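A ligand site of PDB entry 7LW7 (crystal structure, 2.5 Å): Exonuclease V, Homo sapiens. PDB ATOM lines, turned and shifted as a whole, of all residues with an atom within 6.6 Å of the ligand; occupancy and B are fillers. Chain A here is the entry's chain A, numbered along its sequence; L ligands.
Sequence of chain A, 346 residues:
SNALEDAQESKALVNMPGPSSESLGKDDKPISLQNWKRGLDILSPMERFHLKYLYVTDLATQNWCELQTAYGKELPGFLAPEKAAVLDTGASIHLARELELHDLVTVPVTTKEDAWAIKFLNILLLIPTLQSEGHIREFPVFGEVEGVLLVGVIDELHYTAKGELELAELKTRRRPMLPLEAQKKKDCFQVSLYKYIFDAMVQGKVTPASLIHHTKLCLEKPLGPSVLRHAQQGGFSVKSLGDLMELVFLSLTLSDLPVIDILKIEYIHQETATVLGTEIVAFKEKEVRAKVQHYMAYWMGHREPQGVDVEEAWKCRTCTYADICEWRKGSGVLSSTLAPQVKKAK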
ATOM      1  N   TRP A  64     -11.400 -18.847 -15.366  1.00  0.00           N
ATOM      2  CA  TRP A  64     -12.203 -19.385 -16.467  1.00  0.00           C
ATOM      3  C   TRP A  64     -13.451 -18.546 -16.688  1.00  0.00           C
ATOM      4  O   TRP A  64     -13.676 -18.020 -17.789  1.00  0.00           O
ATOM      5  CB  TRP A  64     -12.577 -20.839 -16.169  1.00  0.00           C
ATOM      6  CG  TRP A  64     -13.370 -21.504 -17.243  1.00  0.00           C
ATOM      7  CD1 TRP A  64     -14.726 -21.599 -17.322  1.00  0.00           C
ATOM      8  CD2 TRP A  64     -12.858 -22.188 -18.395  1.00  0.00           C
ATOM      9  NE1 TRP A  64     -15.101 -22.291 -18.452  1.00  0.00           N
ATOM     10  CE2 TRP A  64     -13.965 -22.664 -19.127  1.00  0.00           C
ATOM     11  CE3 TRP A  64     -11.572 -22.444 -18.872  1.00  0.00           C
ATOM     12  CZ2 TRP A  64     -13.820 -23.374 -20.316  1.00  0.00           C
ATOM     13  CZ3 TRP A  64     -11.426 -23.144 -20.059  1.00  0.00           C
ATOM     14  CH2 TRP A  64     -12.555 -23.610 -20.768  1.00  0.00           C
ATOM     15  N   CYS A  65     -14.281 -18.420 -15.658  1.00  0.00           N
ATOM     16  CA  CYS A  65     -15.382 -17.445 -15.665  1.00  0.00           C
ATOM     17  C   CYS A  65     -15.692 -17.078 -14.223  1.00  0.00           C
ATOM     18  O   CYS A  65     -15.971 -17.957 -13.405  1.00  0.00           O
ATOM     19  CB  CYS A  65     -16.636 -17.993 -16.350  1.00  0.00           C
ATOM     20  SG  CYS A  65     -18.058 -16.849 -16.230  1.00  0.00           S
ATOM     21  N   GLU A  66     -15.629 -15.775 -13.930  1.00  0.00           N
ATOM     22  CA  GLU A  66     -15.880 -15.311 -12.578  1.00  0.00           C
ATOM     23  C   GLU A  66     -17.337 -15.512 -12.184  1.00  0.00           C
ATOM     24  O   GLU A  66     -17.642 -15.904 -11.053  1.00  0.00           O
ATOM     25  CB  GLU A  66     -15.483 -13.848 -12.454  1.00  0.00           C
ATOM     26  CG  GLU A  66     -15.805 -13.210 -11.123  1.00  0.00           C
ATOM     27  CD  GLU A  66     -15.136 -11.863 -10.965  1.00  0.00           C
ATOM     28  OE1 GLU A  66     -14.092 -11.800 -10.282  1.00  0.00           O
ATOM     29  OE2 GLU A  66     -15.638 -10.872 -11.540  1.00  0.00           O
ATOM     30  N   LEU A  67     -18.259 -15.249 -13.114  1.00  0.00           N
ATOM     31  CA  LEU A  67     -19.685 -15.448 -12.837  1.00  0.00           C
ATOM     32  C   LEU A  67     -19.989 -16.914 -12.577  1.00  0.00           C
ATOM     33  O   LEU A  67     -20.789 -17.247 -11.697  1.00  0.00           O
ATOM     34  CB  LEU A  67     -20.512 -14.908 -13.997  1.00  0.00           C
ATOM     35  CG  LEU A  67     -21.862 -14.275 -13.697  1.00  0.00           C
ATOM     36  CD1 LEU A  67     -21.843 -13.518 -12.388  1.00  0.00           C
ATOM     37  CD2 LEU A  67     -22.247 -13.359 -14.834  1.00  0.00           C
ATOM     38  N   GLN A  68     -19.360 -17.808 -13.351  1.00  0.00           N
ATOM     39  CA  GLN A  68     -19.570 -19.235 -13.153  1.00  0.00           C
ATOM     40  C   GLN A  68     -19.081 -19.677 -11.781  1.00  0.00           C
ATOM     41  O   GLN A  68     -19.715 -20.523 -11.132  1.00  0.00           O
ATOM     42  CB  GLN A  68     -18.874 -20.016 -14.267  1.00  0.00           C
ATOM     43  CG  GLN A  68     -18.991 -21.531 -14.167  1.00  0.00           C
ATOM     44  CD  GLN A  68     -18.332 -22.229 -15.338  1.00  0.00           C
ATOM     45  OE1 GLN A  68     -17.240 -22.795 -15.200  1.00  0.00           O
ATOM     46  NE2 GLN A  68     -18.984 -22.197 -16.492  1.00  0.00           N
ATOM     47  N   THR A  69     -17.964 -19.123 -11.322  1.00  0.00           N
ATOM     48  CA  THR A  69     -17.484 -19.428  -9.976  1.00  0.00           C
ATOM     49  C   THR A  69     -18.434 -18.874  -8.927  1.00  0.00           C
ATOM     50  O   THR A  69     -18.664 -19.514  -7.894  1.00  0.00           O
ATOM     51  CB  THR A  69     -16.084 -18.857  -9.780  1.00  0.00           C
ATOM     52  OG1 THR A  69     -15.259 -19.226 -10.890  1.00  0.00           O
ATOM     53  CG2 THR A  69     -15.463 -19.392  -8.493  1.00  0.00           C
ATOM     54  N   TYR A  71     -21.768 -18.389  -9.276  1.00  0.00           N
ATOM     55  CA  TYR A  71     -22.926 -19.281  -9.259  1.00  0.00           C
ATOM     56  C   TYR A  71     -22.598 -20.602  -8.582  1.00  0.00           C
ATOM     57  O   TYR A  71     -23.475 -21.207  -7.945  1.00  0.00           O
ATOM     58  CB  TYR A  71     -23.422 -19.532 -10.684  1.00  0.00           C
ATOM     59  CG  TYR A  71     -24.187 -18.385 -11.302  1.00  0.00           C
ATOM     60  CD1 TYR A  71     -25.317 -17.871 -10.692  1.00  0.00           C
ATOM     61  CD2 TYR A  71     -23.780 -17.831 -12.508  1.00  0.00           C
ATOM     62  CE1 TYR A  71     -26.029 -16.828 -11.266  1.00  0.00           C
ATOM     63  CE2 TYR A  71     -24.474 -16.788 -13.091  1.00  0.00           C
ATOM     64  CZ  TYR A  71     -25.597 -16.287 -12.465  1.00  0.00           C
ATOM     65  OH  TYR A  71     -26.296 -15.246 -13.035  1.00  0.00           O
ATOM     66  N   GLN A 306     -17.929 -10.513 -13.163  1.00  0.00           N
ATOM     67  CA  GLN A 306     -17.838 -10.409 -14.606  1.00  0.00           C
ATOM     68  C   GLN A 306     -18.023 -11.770 -15.248  1.00  0.00           C
ATOM     69  O   GLN A 306     -17.552 -12.790 -14.730  1.00  0.00           O
ATOM     70  CB  GLN A 306     -16.480  -9.827 -15.023  1.00  0.00           C
ATOM     71  CG  GLN A 306     -16.190  -8.445 -14.464  1.00  0.00           C
ATOM     72  CD  GLN A 306     -17.149  -7.401 -14.994  1.00  0.00           C
ATOM     73  OE1 GLN A 306     -18.179  -7.124 -14.368  1.00  0.00           O
ATOM     74  NE2 GLN A 306     -16.820  -6.818 -16.133  1.00  0.00           N
ATOM     75  N   GLY A 307     -18.707 -11.786 -16.396  1.00  0.00           N
ATOM     76  CA  GLY A 307     -18.820 -12.967 -17.219  1.00  0.00           C
ATOM     77  C   GLY A 307     -17.656 -13.088 -18.188  1.00  0.00           C
ATOM     78  O   GLY A 307     -16.676 -12.351 -18.124  1.00  0.00           O
ATOM     79  N   VAL A 308     -17.778 -14.051 -19.111  1.00  0.00           N
ATOM     80  CA  VAL A 308     -16.701 -14.276 -20.069  1.00  0.00           C
ATOM     81  C   VAL A 308     -16.693 -13.181 -21.128  1.00  0.00           C
ATOM     82  O   VAL A 308     -17.700 -12.516 -21.391  1.00  0.00           O
ATOM     83  CB  VAL A 308     -16.822 -15.665 -20.713  1.00  0.00           C
ATOM     84  CG1 VAL A 308     -16.932 -16.748 -19.657  1.00  0.00           C
ATOM     85  CG2 VAL A 308     -18.015 -15.713 -21.670  1.00  0.00           C
ATOM     86  N   GLU A 312     -14.916 -15.551 -25.968  1.00  0.00           N
ATOM     87  CA  GLU A 312     -14.981 -16.839 -25.293  1.00  0.00           C
ATOM     88  C   GLU A 312     -16.409 -17.196 -24.899  1.00  0.00           C
ATOM     89  O   GLU A 312     -16.628 -17.865 -23.888  1.00  0.00           O
ATOM     90  CB  GLU A 312     -14.055 -16.841 -24.065  1.00  0.00           C
ATOM     91  CG  GLU A 312     -12.579 -16.889 -24.426  1.00  0.00           C
ATOM     92  CD  GLU A 312     -11.692 -16.998 -23.199  1.00  0.00           C
ATOM     93  OE1 GLU A 312     -12.078 -16.467 -22.141  1.00  0.00           O
ATOM     94  OE2 GLU A 312     -10.613 -17.619 -23.305  1.00  0.00           O
ATOM     95  N   ALA A 313     -17.382 -16.752 -25.699  1.00  0.00           N
ATOM     96  CA  ALA A 313     -18.768 -17.115 -25.441  1.00  0.00           C
ATOM     97  C   ALA A 313     -19.021 -18.608 -25.609  1.00  0.00           C
ATOM     98  O   ALA A 313     -20.080 -19.088 -25.208  1.00  0.00           O
ATOM     99  CB  ALA A 313     -19.692 -16.334 -26.369  1.00  0.00           C
ATOM    100  N   LYS A 315     -17.527 -20.820 -23.919  1.00  0.00           N
ATOM    101  CA  LYS A 315     -17.515 -21.379 -22.571  1.00  0.00           C
ATOM    102  C   LYS A 315     -18.921 -21.577 -22.032  1.00  0.00           C
ATOM    103  O   LYS A 315     -19.156 -22.498 -21.234  1.00  0.00           O
ATOM    104  CB  LYS A 315     -16.715 -20.472 -21.635  1.00  0.00           C
ATOM    105  CG  LYS A 315     -15.228 -20.422 -21.914  1.00  0.00           C
ATOM    106  CD  LYS A 315     -14.519 -19.538 -20.891  1.00  0.00           C
ATOM    107  CE  LYS A 315     -13.029 -19.458 -21.166  1.00  0.00           C
ATOM    108  NZ  LYS A 315     -12.375 -18.396 -20.352  1.00  0.00           N
ATOM    109  N   CYS A 316     -19.871 -20.752 -22.462  1.00  0.00           N
ATOM    110  CA  CYS A 316     -21.241 -20.862 -21.992  1.00  0.00           C
ATOM    111  C   CYS A 316     -21.982 -22.047 -22.593  1.00  0.00           C
ATOM    112  O   CYS A 316     -23.046 -22.411 -22.076  1.00  0.00           O
ATOM    113  CB  CYS A 316     -21.995 -19.566 -22.313  1.00  0.00           C
ATOM    114  SG  CYS A 316     -21.067 -18.043 -21.943  1.00  0.00           S
ATOM    115  N   ARG A 317     -21.442 -22.656 -23.652  1.00  0.00           N
ATOM    116  CA  ARG A 317     -22.112 -23.805 -24.270  1.00  0.00           C
ATOM    117  C   ARG A 317     -22.298 -24.951 -23.291  1.00  0.00           C
ATOM    118  O   ARG A 317     -23.294 -25.674 -23.367  1.00  0.00           O
ATOM    119  CB  ARG A 317     -21.326 -24.276 -25.494  1.00  0.00           C
ATOM    120  CG  ARG A 317     -21.300 -23.299 -26.665  1.00  0.00           C
ATOM    121  CD  ARG A 317     -20.177 -23.639 -27.634  1.00  0.00           C
ATOM    122  NE  ARG A 317     -20.590 -23.496 -29.034  1.00  0.00           N
ATOM    123  CZ  ARG A 317     -20.708 -24.511 -29.879  1.00  0.00           C
ATOM    124  NH1 ARG A 317     -20.432 -25.745 -29.488  1.00  0.00           N
ATOM    125  NH2 ARG A 317     -21.093 -24.279 -31.140  1.00  0.00           N
ATOM    126  N   CYS A 319     -21.852 -24.581 -19.740  1.00  0.00           N
ATOM    127  CA  CYS A 319     -21.922 -24.023 -18.392  1.00  0.00           C
ATOM    128  C   CYS A 319     -23.276 -24.340 -17.766  1.00  0.00           C
ATOM    129  O   CYS A 319     -24.315 -24.069 -18.374  1.00  0.00           O
ATOM    130  CB  CYS A 319     -21.691 -22.510 -18.425  1.00  0.00           C
ATOM    131  SG  CYS A 319     -22.102 -21.712 -16.859  1.00  0.00           S
ATOM    132  N   THR A 320     -23.254 -24.881 -16.555  1.00  0.00           N
ATOM    133  CA  THR A 320     -24.483 -25.329 -15.893  1.00  0.00           C
ATOM    134  C   THR A 320     -25.488 -24.194 -15.746  1.00  0.00           C
ATOM    135  O   THR A 320     -26.704 -24.399 -15.871  1.00  0.00           O
ATOM    136  CB  THR A 320     -24.151 -25.925 -14.531  1.00  0.00           C
ATOM    137  OG1 THR A 320     -23.265 -27.035 -14.693  1.00  0.00           O
ATOM    138  CG2 THR A 320     -25.423 -26.405 -13.819  1.00  0.00           C
ATOM    139  N   TYR A 321     -25.008 -22.969 -15.507  1.00  0.00           N
ATOM    140  CA  TYR A 321     -25.863 -21.833 -15.196  1.00  0.00           C
ATOM    141  C   TYR A 321     -26.147 -20.968 -16.416  1.00  0.00           C
ATOM    142  O   TYR A 321     -26.440 -19.776 -16.285  1.00  0.00           O
ATOM    143  CB  TYR A 321     -25.231 -21.005 -14.077  1.00  0.00           C
ATOM    144  CG  TYR A 321     -24.671 -21.846 -12.956  1.00  0.00           C
ATOM    145  CD1 TYR A 321     -23.324 -22.162 -12.909  1.00  0.00           C
ATOM    146  CD2 TYR A 321     -25.500 -22.326 -11.944  1.00  0.00           C
ATOM    147  CE1 TYR A 321     -22.807 -22.934 -11.877  1.00  0.00           C
ATOM    148  CE2 TYR A 321     -24.996 -23.096 -10.917  1.00  0.00           C
ATOM    149  CZ  TYR A 321     -23.648 -23.400 -10.891  1.00  0.00           C
ATOM    150  OH  TYR A 321     -23.144 -24.170  -9.864  1.00  0.00           O
ATOM    151  N   ALA A 322     -26.082 -21.546 -17.618  1.00  0.00           N
ATOM    152  CA  ALA A 322     -26.298 -20.760 -18.831  1.00  0.00           C
ATOM    153  C   ALA A 322     -27.742 -20.291 -18.948  1.00  0.00           C
ATOM    154  O   ALA A 322     -27.994 -19.234 -19.544  1.00  0.00           O
ATOM    155  CB  ALA A 322     -25.909 -21.582 -20.062  1.00  0.00           C
ATOM    156  N   ASP A 323     -28.690 -21.048 -18.396  1.00  0.00           N
ATOM    157  CA  ASP A 323     -30.104 -20.715 -18.509  1.00  0.00           C
ATOM    158  C   ASP A 323     -30.576 -19.727 -17.454  1.00  0.00           C
ATOM    159  O   ASP A 323     -31.757 -19.376 -17.442  1.00  0.00           O
ATOM    160  CB  ASP A 323     -30.952 -21.996 -18.428  1.00  0.00           C
ATOM    161  CG  ASP A 323     -30.629 -22.836 -17.200  1.00  0.00           C
ATOM    162  OD1 ASP A 323     -31.478 -23.653 -16.801  1.00  0.00           O
ATOM    163  OD2 ASP A 323     -29.529 -22.660 -16.637  1.00  0.00           O
ATOM    164  N   CYS A 325     -28.021 -17.107 -16.478  1.00  0.00           N
ATOM    165  CA  CYS A 325     -26.985 -16.089 -16.500  1.00  0.00           C
ATOM    166  C   CYS A 325     -27.470 -14.879 -17.279  1.00  0.00           C
ATOM    167  O   CYS A 325     -27.796 -14.989 -18.467  1.00  0.00           O
ATOM    168  CB  CYS A 325     -25.712 -16.659 -17.113  1.00  0.00           C
ATOM    169  SG  CYS A 325     -24.309 -15.537 -17.082  1.00  0.00           S
ATOM    170  N   GLU A 326     -27.509 -13.719 -16.623  1.00  0.00           N
ATOM    171  CA  GLU A 326     -27.881 -12.475 -17.293  1.00  0.00           C
ATOM    172  C   GLU A 326     -26.765 -11.925 -18.162  1.00  0.00           C
ATOM    173  O   GLU A 326     -27.037 -11.143 -19.087  1.00  0.00           O
ATOM    174  CB  GLU A 326     -28.292 -11.420 -16.255  1.00  0.00           C
ATOM    175  CG  GLU A 326     -29.029 -11.988 -15.056  1.00  0.00           C
ATOM    176  CD  GLU A 326     -30.521 -12.079 -15.271  1.00  0.00           C
ATOM    177  OE1 GLU A 326     -31.260 -12.271 -14.281  1.00  0.00           O
ATOM    178  OE2 GLU A 326     -30.969 -11.946 -16.429  1.00  0.00           O
ATOM    179  N   TRP A 327     -25.515 -12.294 -17.883  1.00  0.00           N
ATOM    180  CA  TRP A 327     -24.399 -11.908 -18.740  1.00  0.00           C
ATOM    181  C   TRP A 327     -24.512 -12.574 -20.109  1.00  0.00           C
ATOM    182  O   TRP A 327     -24.191 -11.965 -21.137  1.00  0.00           O
ATOM    183  CB  TRP A 327     -23.082 -12.280 -18.064  1.00  0.00           C
ATOM    184  CG  TRP A 327     -21.858 -11.751 -18.719  1.00  0.00           C
ATOM    185  CD1 TRP A 327     -21.219 -12.265 -19.810  1.00  0.00           C
ATOM    186  CD2 TRP A 327     -21.093 -10.613 -18.310  1.00  0.00           C
ATOM    187  NE1 TRP A 327     -20.111 -11.520 -20.114  1.00  0.00           N
ATOM    188  CE2 TRP A 327     -20.005 -10.493 -19.204  1.00  0.00           C
ATOM    189  CE3 TRP A 327     -21.215  -9.681 -17.270  1.00  0.00           C
ATOM    190  CZ2 TRP A 327     -19.058  -9.484 -19.093  1.00  0.00           C
ATOM    191  CZ3 TRP A 327     -20.274  -8.680 -17.169  1.00  0.00           C
ATOM    192  CH2 TRP A 327     -19.203  -8.588 -18.072  1.00  0.00           C
ATOM    193  N   ARG A 328     -24.955 -13.842 -20.137  1.00  0.00           N
ATOM    194  CA  ARG A 328     -25.113 -14.561 -21.392  1.00  0.00           C
ATOM    195  C   ARG A 328     -26.123 -13.873 -22.307  1.00  0.00           C
ATOM    196  O   ARG A 328     -26.011 -13.964 -23.539  1.00  0.00           O
ATOM    197  CB  ARG A 328     -25.544 -16.005 -21.120  1.00  0.00           C
ATOM    198  CG  ARG A 328     -25.065 -17.007 -22.159  1.00  0.00           C
ATOM    199  CD  ARG A 328     -26.157 -18.009 -22.492  1.00  0.00           C
ATOM    200  NE  ARG A 328     -25.712 -19.006 -23.467  1.00  0.00           N
ATOM    201  CZ  ARG A 328     -25.348 -18.725 -24.717  1.00  0.00           C
ATOM    202  NH1 ARG A 328     -25.381 -17.480 -25.159  1.00  0.00           N
ATOM    203  NH2 ARG A 328     -24.953 -19.699 -25.526  1.00  0.00           N
HETATM  204 FE1  LIG L   1     -21.755 -19.558 -17.482  1.00  0.00          FE
HETATM  205 FE2  LIG L   1     -21.150 -18.032 -19.675  1.00  0.00          FE
HETATM  206 FE3  LIG L   1     -20.005 -17.486 -17.256  1.00  0.00          FE
HETATM  207 FE4  LIG L   1     -22.659 -16.996 -17.660  1.00  0.00          FE
HETATM  208  S1  LIG L   1     -20.925 -15.989 -18.715  1.00  0.00           S
HETATM  209  S2  LIG L   1     -21.718 -17.998 -15.842  1.00  0.00           S
HETATM  210  S3  LIG L   1     -23.221 -18.733 -19.016  1.00  0.00           S
HETATM  211  S4  LIG L   1     -19.716 -19.362 -18.497  1.00  0.00           S
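SG of Cys 319 binds FE1 of the ligand (2.3 Å). The side-chain sulfur (SG) of Cys 316 is bound to an iron atom (FE2) of the ligand, 2.3 Å away. The side-chain sulfur (SG) of Cys 325 is bound to an iron atom (FE4) of the ligand. SG of Cys 65 is bound to FE3 of the ligand (2.3 Å). S2 of the ligand lies close to N of Gln 68 (3.4 Å). The side-chain amide nitrogen (NE2) of Gln 68 sits close to a sulfur (S4) of the ligand, 3.5 Å away. N of Val 308 sits close to S1 of the ligand, 3.7 Å away.
The side-chain amide nitrogen (NE2) of Gln 68 sits close to the side-chain sulfur (SG) of Cys 319. The backbone NH (N) of Tyr 321 sits close to the side-chain sulfur (SG) of Cys 319, 3.4 Å away. SG of Cys 325 lies close to N of Trp 327 (3.6 Å). The side-chain sulfur (SG) of Cys 325 sits close to the backbone NH (N) of Arg 328, 3.6 Å away. SG of Cys 65 lies close to N of Leu 67 (3.5 Å). The backbone carbonyl oxygen of Cys 65 is in hydrogen-bond range of the side-chain hydroxyl of Thr 69 (2.9 Å). The backbone carbonyl oxygen (O) of Val 308 is in hydrogen-bond range of the indole nitrogen (NE1) of Trp 327, 2.9 Å away. O of Gln 306 is in hydrogen-bond range of N of Leu 67 (3.0 Å).
Merely in contact with the ligand: Ala 322 (3.7 Å), Leu 67 (3.8 Å), Trp 327 (3.9 Å), Tyr 71 (3.9 Å) and Gly 307 (3.98 Å). Hydrophobic or aromatic side chains within 4 Å of the ligand: Leu 67, Tyr 71, Val 308 and Trp 327. 11 residues have an atom within 4 Å of the ligand: Cys 65, Leu 67, Gln 68, Tyr 71, Gly 307, Val 308, Cys 316, Cys 319, Ala 322, Cys 325 and Trp 327.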
